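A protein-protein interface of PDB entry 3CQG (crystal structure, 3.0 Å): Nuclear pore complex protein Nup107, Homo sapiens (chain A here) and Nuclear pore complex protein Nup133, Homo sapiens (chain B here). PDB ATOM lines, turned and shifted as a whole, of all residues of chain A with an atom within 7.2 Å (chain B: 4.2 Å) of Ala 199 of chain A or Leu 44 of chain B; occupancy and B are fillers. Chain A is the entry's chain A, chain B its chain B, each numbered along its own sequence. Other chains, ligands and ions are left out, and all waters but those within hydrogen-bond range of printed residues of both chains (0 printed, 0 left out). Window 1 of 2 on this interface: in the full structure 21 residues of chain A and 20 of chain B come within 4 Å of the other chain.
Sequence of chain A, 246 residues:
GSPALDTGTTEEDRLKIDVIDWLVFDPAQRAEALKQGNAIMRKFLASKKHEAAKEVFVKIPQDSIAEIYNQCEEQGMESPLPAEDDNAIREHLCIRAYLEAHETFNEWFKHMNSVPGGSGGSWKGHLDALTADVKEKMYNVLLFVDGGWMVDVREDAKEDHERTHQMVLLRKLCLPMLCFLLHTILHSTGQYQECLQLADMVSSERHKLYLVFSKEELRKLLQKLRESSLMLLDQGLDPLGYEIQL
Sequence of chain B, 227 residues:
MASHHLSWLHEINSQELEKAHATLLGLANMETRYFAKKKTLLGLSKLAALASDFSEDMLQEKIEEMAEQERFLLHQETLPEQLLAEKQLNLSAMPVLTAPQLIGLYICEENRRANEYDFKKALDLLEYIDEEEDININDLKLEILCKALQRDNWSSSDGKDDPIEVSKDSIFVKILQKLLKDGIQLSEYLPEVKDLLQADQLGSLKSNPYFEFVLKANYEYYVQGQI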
ATOM      1  N   GLU A 194     -12.216  -2.454  21.560  1.00  0.00           N
ATOM      2  CA  GLU A 194     -12.216  -1.436  22.601  1.00  0.00           C
ATOM      3  C   GLU A 194     -11.023  -1.618  23.519  1.00  0.00           C
ATOM      4  O   GLU A 194     -10.462  -0.653  24.041  1.00  0.00           O
ATOM      5  CB  GLU A 194     -13.495  -1.521  23.416  1.00  0.00           C
ATOM      6  CG  GLU A 194     -13.685  -0.341  24.336  1.00  0.00           C
ATOM      7  CD  GLU A 194     -15.139  -0.070  24.616  1.00  0.00           C
ATOM      8  OE1 GLU A 194     -15.437   0.542  25.663  1.00  0.00           O
ATOM      9  OE2 GLU A 194     -15.982  -0.474  23.785  1.00  0.00           O
ATOM     10  N   CYS A 195     -10.654  -2.878  23.710  1.00  0.00           N
ATOM     11  CA  CYS A 195      -9.486  -3.243  24.484  1.00  0.00           C
ATOM     12  C   CYS A 195      -8.249  -2.573  23.910  1.00  0.00           C
ATOM     13  O   CYS A 195      -7.415  -2.068  24.650  1.00  0.00           O
ATOM     14  CB  CYS A 195      -9.306  -4.762  24.484  1.00  0.00           C
ATOM     15  SG  CYS A 195     -10.529  -5.677  25.453  1.00  0.00           S
ATOM     16  N   LEU A 196      -8.126  -2.559  22.591  1.00  0.00           N
ATOM     17  CA  LEU A 196      -6.962  -1.935  21.982  1.00  0.00           C
ATOM     18  C   LEU A 196      -7.009  -0.423  22.037  1.00  0.00           C
ATOM     19  O   LEU A 196      -5.985   0.242  21.861  1.00  0.00           O
ATOM     20  CB  LEU A 196      -6.750  -2.408  20.547  1.00  0.00           C
ATOM     21  CG  LEU A 196      -5.971  -3.716  20.537  1.00  0.00           C
ATOM     22  CD1 LEU A 196      -6.810  -4.803  21.186  1.00  0.00           C
ATOM     23  CD2 LEU A 196      -5.609  -4.088  19.137  1.00  0.00           C
ATOM     24  N   GLN A 197      -8.194   0.122  22.274  1.00  0.00           N
ATOM     25  CA  GLN A 197      -8.338   1.560  22.362  1.00  0.00           C
ATOM     26  C   GLN A 197      -8.093   2.033  23.791  1.00  0.00           C
ATOM     27  O   GLN A 197      -8.159   3.226  24.079  1.00  0.00           O
ATOM     28  CB  GLN A 197      -9.710   1.990  21.876  1.00  0.00           C
ATOM     29  CG  GLN A 197      -9.914   1.848  20.391  1.00  0.00           C
ATOM     30  CD  GLN A 197     -11.349   2.122  19.990  1.00  0.00           C
ATOM     31  OE1 GLN A 197     -12.280   1.636  20.627  1.00  0.00           O
ATOM     32  NE2 GLN A 197     -11.536   2.906  18.936  1.00  0.00           N
ATOM     33  N   LEU A 198      -7.806   1.102  24.690  1.00  0.00           N
ATOM     34  CA  LEU A 198      -7.282   1.496  25.979  1.00  0.00           C
ATOM     35  C   LEU A 198      -5.949   2.175  25.749  1.00  0.00           C
ATOM     36  O   LEU A 198      -5.521   2.992  26.546  1.00  0.00           O
ATOM     37  CB  LEU A 198      -7.096   0.293  26.896  1.00  0.00           C
ATOM     38  CG  LEU A 198      -8.347  -0.487  27.284  1.00  0.00           C
ATOM     39  CD1 LEU A 198      -8.019  -1.444  28.398  1.00  0.00           C
ATOM     40  CD2 LEU A 198      -9.465   0.442  27.711  1.00  0.00           C
ATOM     41  N   ALA A 199      -5.294   1.833  24.648  1.00  0.00           N
ATOM     42  CA  ALA A 199      -3.995   2.413  24.331  1.00  0.00           C
ATOM     43  C   ALA A 199      -4.152   3.902  24.075  1.00  0.00           C
ATOM     44  O   ALA A 199      -3.330   4.712  24.485  1.00  0.00           O
ATOM     45  CB  ALA A 199      -3.398   1.732  23.118  1.00  0.00           C
ATOM     46  N   ASP A 200      -5.227   4.247  23.378  1.00  0.00           N
ATOM     47  CA  ASP A 200      -5.633   5.631  23.195  1.00  0.00           C
ATOM     48  C   ASP A 200      -5.814   6.327  24.530  1.00  0.00           C
ATOM     49  O   ASP A 200      -5.303   7.426  24.751  1.00  0.00           O
ATOM     50  CB  ASP A 200      -6.936   5.681  22.408  1.00  0.00           C
ATOM     51  CG  ASP A 200      -6.740   5.290  20.982  1.00  0.00           C
ATOM     52  OD1 ASP A 200      -5.566   5.187  20.594  1.00  0.00           O
ATOM     53  OD2 ASP A 200      -7.736   5.096  20.252  1.00  0.00           O
ATOM     54  N   MET A 201      -6.539   5.664  25.421  1.00  0.00           N
ATOM     55  CA  MET A 201      -6.929   6.243  26.696  1.00  0.00           C
ATOM     56  C   MET A 201      -5.760   6.538  27.630  1.00  0.00           C
ATOM     57  O   MET A 201      -5.704   7.595  28.263  1.00  0.00           O
ATOM     58  CB  MET A 201      -7.902   5.307  27.390  1.00  0.00           C
ATOM     59  CG  MET A 201      -8.316   5.801  28.728  1.00  0.00           C
ATOM     60  SD  MET A 201      -9.498   4.681  29.470  1.00  0.00           S
ATOM     61  CE  MET A 201      -8.436   3.301  29.852  1.00  0.00           C
ATOM     62  N   VAL A 202      -4.839   5.591  27.718  1.00  0.00           N
ATOM     63  CA  VAL A 202      -3.735   5.696  28.648  1.00  0.00           C
ATOM     64  C   VAL A 202      -2.663   6.667  28.180  1.00  0.00           C
ATOM     65  O   VAL A 202      -2.027   7.330  28.993  1.00  0.00           O
ATOM     66  CB  VAL A 202      -3.105   4.324  28.893  1.00  0.00           C
ATOM     67  CG1 VAL A 202      -1.884   4.450  29.774  1.00  0.00           C
ATOM     68  CG2 VAL A 202      -4.134   3.385  29.497  1.00  0.00           C
ATOM     69  N   SER A 203      -2.459   6.756  26.871  1.00  0.00           N
ATOM     70  CA  SER A 203      -1.374   7.567  26.327  1.00  0.00           C
ATOM     71  C   SER A 203      -1.878   8.950  25.967  1.00  0.00           C
ATOM     72  O   SER A 203      -1.101   9.838  25.627  1.00  0.00           O
ATOM     73  CB  SER A 203      -0.772   6.907  25.089  1.00  0.00           C
ATOM     74  OG  SER A 203      -1.621   7.089  23.971  1.00  0.00           O
ATOM     75  N   SER A 204      -3.192   9.117  26.036  1.00  0.00           N
ATOM     76  CA  SER A 204      -3.828  10.389  25.743  1.00  0.00           C
ATOM     77  C   SER A 204      -3.157  11.493  26.527  1.00  0.00           C
ATOM     78  O   SER A 204      -2.961  11.363  27.729  1.00  0.00           O
ATOM     79  CB  SER A 204      -5.305  10.324  26.124  1.00  0.00           C
ATOM     80  OG  SER A 204      -6.026  11.408  25.568  1.00  0.00           O
ATOM     81  N   LEU A 221       0.297  -4.148  30.461  1.00  0.00           N
ATOM     82  CA  LEU A 221      -0.819  -3.649  29.664  1.00  0.00           C
ATOM     83  C   LEU A 221      -0.644  -3.999  28.194  1.00  0.00           C
ATOM     84  O   LEU A 221      -1.553  -4.534  27.568  1.00  0.00           O
ATOM     85  CB  LEU A 221      -0.981  -2.137  29.833  1.00  0.00           C
ATOM     86  CG  LEU A 221      -2.027  -1.442  28.953  1.00  0.00           C
ATOM     87  CD1 LEU A 221      -3.440  -1.753  29.423  1.00  0.00           C
ATOM     88  CD2 LEU A 221      -1.795   0.052  28.934  1.00  0.00           C
ATOM     89  N   LEU A 222       0.534  -3.707  27.654  1.00  0.00           N
ATOM     90  CA  LEU A 222       0.893  -4.076  26.284  1.00  0.00           C
ATOM     91  C   LEU A 222       0.673  -5.554  25.962  1.00  0.00           C
ATOM     92  O   LEU A 222       0.153  -5.899  24.914  1.00  0.00           O
ATOM     93  CB  LEU A 222       2.359  -3.734  26.036  1.00  0.00           C
ATOM     94  CG  LEU A 222       2.756  -2.261  26.102  1.00  0.00           C
ATOM     95  CD1 LEU A 222       4.262  -2.123  26.218  1.00  0.00           C
ATOM     96  CD2 LEU A 222       2.234  -1.537  24.880  1.00  0.00           C
ATOM     97  N   LEU A 225      -2.973  -6.626  25.617  1.00  0.00           N
ATOM     98  CA  LEU A 225      -3.619  -6.132  24.414  1.00  0.00           C
ATOM     99  C   LEU A 225      -3.213  -6.988  23.231  1.00  0.00           C
ATOM    100  O   LEU A 225      -3.953  -7.105  22.246  1.00  0.00           O
ATOM    101  CB  LEU A 225      -3.252  -4.668  24.153  1.00  0.00           C
ATOM    102  CG  LEU A 225      -3.703  -3.658  25.207  1.00  0.00           C
ATOM    103  CD1 LEU A 225      -3.539  -2.230  24.715  1.00  0.00           C
ATOM    104  CD2 LEU A 225      -5.143  -3.927  25.610  1.00  0.00           C
ATOM    105  N   ARG A 226      -2.026  -7.576  23.327  1.00  0.00           N
ATOM    106  CA  ARG A 226      -1.591  -8.538  22.331  1.00  0.00           C
ATOM    107  C   ARG A 226      -2.588  -9.685  22.307  1.00  0.00           C
ATOM    108  O   ARG A 226      -3.126 -10.028  21.263  1.00  0.00           O
ATOM    109  CB  ARG A 226      -0.193  -9.047  22.666  1.00  0.00           C
ATOM    110  CG  ARG A 226       0.468  -9.859  21.571  1.00  0.00           C
ATOM    111  CD  ARG A 226       1.652 -10.619  22.132  1.00  0.00           C
ATOM    112  NE  ARG A 226       2.353 -11.379  21.105  1.00  0.00           N
ATOM    113  CZ  ARG A 226       1.948 -12.557  20.645  1.00  0.00           C
ATOM    114  NH1 ARG A 226       0.841 -13.104  21.122  1.00  0.00           N
ATOM    115  NH2 ARG A 226       2.649 -13.182  19.706  1.00  0.00           N
ATOM    116  N   SER A 229      -5.308  -8.688  20.204  1.00  0.00           N
ATOM    117  CA  SER A 229      -5.107  -8.647  18.751  1.00  0.00           C
ATOM    118  C   SER A 229      -5.066 -10.046  18.134  1.00  0.00           C
ATOM    119  O   SER A 229      -5.481 -10.241  16.993  1.00  0.00           O
ATOM    120  CB  SER A 229      -3.839  -7.876  18.391  1.00  0.00           C
ATOM    121  OG  SER A 229      -3.989  -6.513  18.718  1.00  0.00           O
ATOM    122  N   PRO A 239      -5.048  -6.303  13.310  1.00  0.00           N
ATOM    123  CA  PRO A 239      -4.788  -6.481  14.742  1.00  0.00           C
ATOM    124  C   PRO A 239      -5.619  -5.530  15.613  1.00  0.00           C
ATOM    125  O   PRO A 239      -5.844  -5.816  16.795  1.00  0.00           O
ATOM    126  CB  PRO A 239      -3.294  -6.154  14.868  1.00  0.00           C
ATOM    127  CG  PRO A 239      -2.748  -6.306  13.495  1.00  0.00           C
ATOM    128  CD  PRO A 239      -3.843  -5.870  12.586  1.00  0.00           C
ATOM    129  N   LEU A 240      -6.071  -4.423  15.026  1.00  0.00           N
ATOM    130  CA  LEU A 240      -6.815  -3.402  15.752  1.00  0.00           C
ATOM    131  C   LEU A 240      -8.311  -3.562  15.541  1.00  0.00           C
ATOM    132  O   LEU A 240      -9.102  -2.731  15.975  1.00  0.00           O
ATOM    133  CB  LEU A 240      -6.369  -2.006  15.321  1.00  0.00           C
ATOM    134  CG  LEU A 240      -5.192  -1.386  16.073  1.00  0.00           C
ATOM    135  CD1 LEU A 240      -4.004  -2.336  16.166  1.00  0.00           C
ATOM    136  CD2 LEU A 240      -4.795  -0.076  15.420  1.00  0.00           C
ATOM    137  N   LEU B  24       5.344   0.232  14.976  1.00  0.00           N
ATOM    138  CA  LEU B  24       4.063   0.834  15.349  1.00  0.00           C
ATOM    139  C   LEU B  24       3.951   2.305  14.940  1.00  0.00           C
ATOM    140  O   LEU B  24       2.947   2.712  14.364  1.00  0.00           O
ATOM    141  CB  LEU B  24       3.778   0.660  16.849  1.00  0.00           C
ATOM    142  CG  LEU B  24       3.004  -0.612  17.211  1.00  0.00           C
ATOM    143  CD1 LEU B  24       2.773  -0.734  18.703  1.00  0.00           C
ATOM    144  CD2 LEU B  24       1.687  -0.647  16.484  1.00  0.00           C
ATOM    145  N   THR B  40      -5.210   4.880  17.471  1.00  0.00           N
ATOM    146  CA  THR B  40      -4.813   3.765  18.312  1.00  0.00           C
ATOM    147  C   THR B  40      -3.345   3.388  18.117  1.00  0.00           C
ATOM    148  O   THR B  40      -2.583   3.280  19.078  1.00  0.00           O
ATOM    149  CB  THR B  40      -5.696   2.527  18.070  1.00  0.00           C
ATOM    150  OG1 THR B  40      -7.082   2.877  18.189  1.00  0.00           O
ATOM    151  CG2 THR B  40      -5.371   1.454  19.077  1.00  0.00           C
ATOM    152  N   LEU B  41      -2.952   3.189  16.867  1.00  0.00           N
ATOM    153  CA  LEU B  41      -1.579   2.799  16.554  1.00  0.00           C
ATOM    154  C   LEU B  41      -0.568   3.756  17.149  1.00  0.00           C
ATOM    155  O   LEU B  41       0.461   3.335  17.666  1.00  0.00           O
ATOM    156  CB  LEU B  41      -1.374   2.722  15.043  1.00  0.00           C
ATOM    157  CG  LEU B  41      -2.022   1.532  14.346  1.00  0.00           C
ATOM    158  CD1 LEU B  41      -1.938   1.738  12.864  1.00  0.00           C
ATOM    159  CD2 LEU B  41      -1.349   0.240  14.761  1.00  0.00           C
ATOM    160  N   LEU B  42      -0.867   5.049  17.056  1.00  0.00           N
ATOM    161  CA  LEU B  42      -0.014   6.090  17.623  1.00  0.00           C
ATOM    162  C   LEU B  42      -0.005   6.054  19.157  1.00  0.00           C
ATOM    163  O   LEU B  42       1.042   6.217  19.781  1.00  0.00           O
ATOM    164  CB  LEU B  42      -0.443   7.476  17.129  1.00  0.00           C
ATOM    165  CG  LEU B  42       0.560   8.604  17.387  1.00  0.00           C
ATOM    166  CD1 LEU B  42       1.579   8.646  16.271  1.00  0.00           C
ATOM    167  CD2 LEU B  42      -0.128   9.950  17.519  1.00  0.00           C
ATOM    168  N   GLY B  43      -1.173   5.849  19.762  1.00  0.00           N
ATOM    169  CA  GLY B  43      -1.239   5.640  21.192  1.00  0.00           C
ATOM    170  C   GLY B  43      -0.424   4.418  21.564  1.00  0.00           C
ATOM    171  O   GLY B  43       0.355   4.435  22.511  1.00  0.00           O
ATOM    172  N   LEU B  44      -0.601   3.350  20.793  1.00  0.00           N
ATOM    173  CA  LEU B  44       0.182   2.126  20.961  1.00  0.00           C
ATOM    174  C   LEU B  44       1.675   2.380  20.828  1.00  0.00           C
ATOM    175  O   LEU B  44       2.472   1.898  21.633  1.00  0.00           O
ATOM    176  CB  LEU B  44      -0.233   1.069  19.937  1.00  0.00           C
ATOM    177  CG  LEU B  44      -1.360   0.091  20.268  1.00  0.00           C
ATOM    178  CD1 LEU B  44      -1.844  -0.601  19.000  1.00  0.00           C
ATOM    179  CD2 LEU B  44      -0.918  -0.926  21.297  1.00  0.00           C
ATOM    180  N   SER B  45       2.048   3.126  19.797  1.00  0.00           N
ATOM    181  CA  SER B  45       3.433   3.494  19.563  1.00  0.00           C
ATOM    182  C   SER B  45       4.014   4.189  20.786  1.00  0.00           C
ATOM    183  O   SER B  45       5.111   3.868  21.235  1.00  0.00           O
ATOM    184  CB  SER B  45       3.514   4.419  18.349  1.00  0.00           C
ATOM    185  OG  SER B  45       4.852   4.751  18.051  1.00  0.00           O
ATOM    186  N   LYS B  46       3.249   5.130  21.332  1.00  0.00           N
ATOM    187  CA  LYS B  46       3.665   5.935  22.481  1.00  0.00           C
ATOM    188  C   LYS B  46       3.800   5.117  23.752  1.00  0.00           C
ATOM    189  O   LYS B  46       4.686   5.365  24.559  1.00  0.00           O
ATOM    190  CB  LYS B  46       2.673   7.073  22.699  1.00  0.00           C
ATOM    191  CG  LYS B  46       2.964   7.971  23.879  1.00  0.00           C
ATOM    192  CD  LYS B  46       2.076   9.198  23.812  1.00  0.00           C
ATOM    193  CE  LYS B  46       2.298  10.137  24.973  1.00  0.00           C
ATOM    194  NZ  LYS B  46       1.558  11.406  24.743  1.00  0.00           N
ATOM    195  N   LEU B  47       2.913   4.149  23.941  1.00  0.00           N
ATOM    196  CA  LEU B  47       3.020   3.255  25.089  1.00  0.00           C
ATOM    197  C   LEU B  47       4.301   2.439  25.023  1.00  0.00           C
ATOM    198  O   LEU B  47       5.019   2.316  26.012  1.00  0.00           O
ATOM    199  CB  LEU B  47       1.816   2.320  25.171  1.00  0.00           C
ATOM    200  CG  LEU B  47       0.470   2.981  25.465  1.00  0.00           C
ATOM    201  CD1 LEU B  47      -0.560   1.929  25.858  1.00  0.00           C
ATOM    202  CD2 LEU B  47       0.599   4.048  26.550  1.00  0.00           C
ATOM    203  N   ALA B  48       4.576   1.878  23.850  1.00  0.00           N
ATOM    204  CA  ALA B  48       5.796   1.112  23.629  1.00  0.00           C
ATOM    205  C   ALA B  48       7.044   1.929  23.991  1.00  0.00           C
ATOM    206  O   ALA B  48       7.895   1.480  24.756  1.00  0.00           O
ATOM    207  CB  ALA B  48       5.854   0.633  22.180  1.00  0.00           C
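Among the printed residues, merely in contact across the chains: Leu 196 of chain A with Thr 40 of chain B (3.1 Å), Ser 203 of chain A with Gly 43 of chain B (3.2 Å), Leu 240 of chain A with Leu 41 of chain B (3.4 Å), Ser 203 of chain A with Leu 47 of chain B (3.5 Å), Gln 197 of chain A with Thr 40 of chain B (3.7 Å), Ala 199 of chain A with Leu 47 of chain B (3.8 Å), Leu 221 of chain A with Leu 47 of chain B (3.8 Å), Leu 240 of chain A with Thr 40 of chain B (3.8 Å), Ala 199 of chain A with Leu 44 of chain B (3.9 Å), Leu 222 of chain A with Leu 47 of chain B (3.9 Å) and Leu 240 of chain A with Leu 44 of chain B (3.96 Å).
The side-chain hydroxyl (OG) of Ser 203 of chain A is in hydrogen-bond range of the backbone carbonyl oxygen (O) of Ala 199 of chain A (3.0 Å).
The side-chain amino group of Lys 46 of chain B is in hydrogen-bond range of the backbone carbonyl oxygen of Ser 203 of chain A (3.2 Å).
OG1 of Thr 40 of chain B lies within hydrogen-bond range of OD2 of Asp 200 of chain A (3.1 Å).
Of the printed residues of chain B, Ala 199 of chain A touches Leu 44 (3.9 Å) and Leu 47 (3.8 Å).
Of the printed residues of chain A, Leu 44 of chain B touches Ala 199 (3.9 Å) and Leu 240 (3.96 Å).
Of the printed residues of chain A, Leu 47 of chain B touches Ala 199 (3.8 Å), Ser 203 (3.5 Å), Leu 221 (3.8 Å) and Leu 222 (3.9 Å).
Of the printed residues of chain B, Ser 203 of chain A touches Gly 43 (3.2 Å), Lys 46 (3.2 Å) and Leu 47 (3.5 Å).
Of the printed residues of chain B, Gln 197 of chain A touches Thr 40.
Of the printed residues of chain B, Leu 222 of chain A touches Leu 47 (3.9 Å).
The nearest printed residue of chain B that does not touch Ala 199 of chain A is Gly 43 of chain B (4.01 Å).
The nearest printed residue of chain B that does not touch Gln 197 of chain A is Leu 44 of chain B (7.1 Å).
Hydrophobic or aromatic side chains of chain B that line the printed part of chain A: Leu 41, Leu 44 and Leu 47.
Of the 18 printed residues of chain A, 8 touch a printed residue of chain B.
Hydrophobic or aromatic side chains of chain A that line the printed part of chain B: Ala 199, Leu 221, Leu 222 and Leu 240.
Among the printed residues, 13 pairs touch across the chains.
Among the printed residues, no Asp or Glu carboxylate lies within 4 Å of a Lys or Arg side-chain nitrogen of the other chain.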
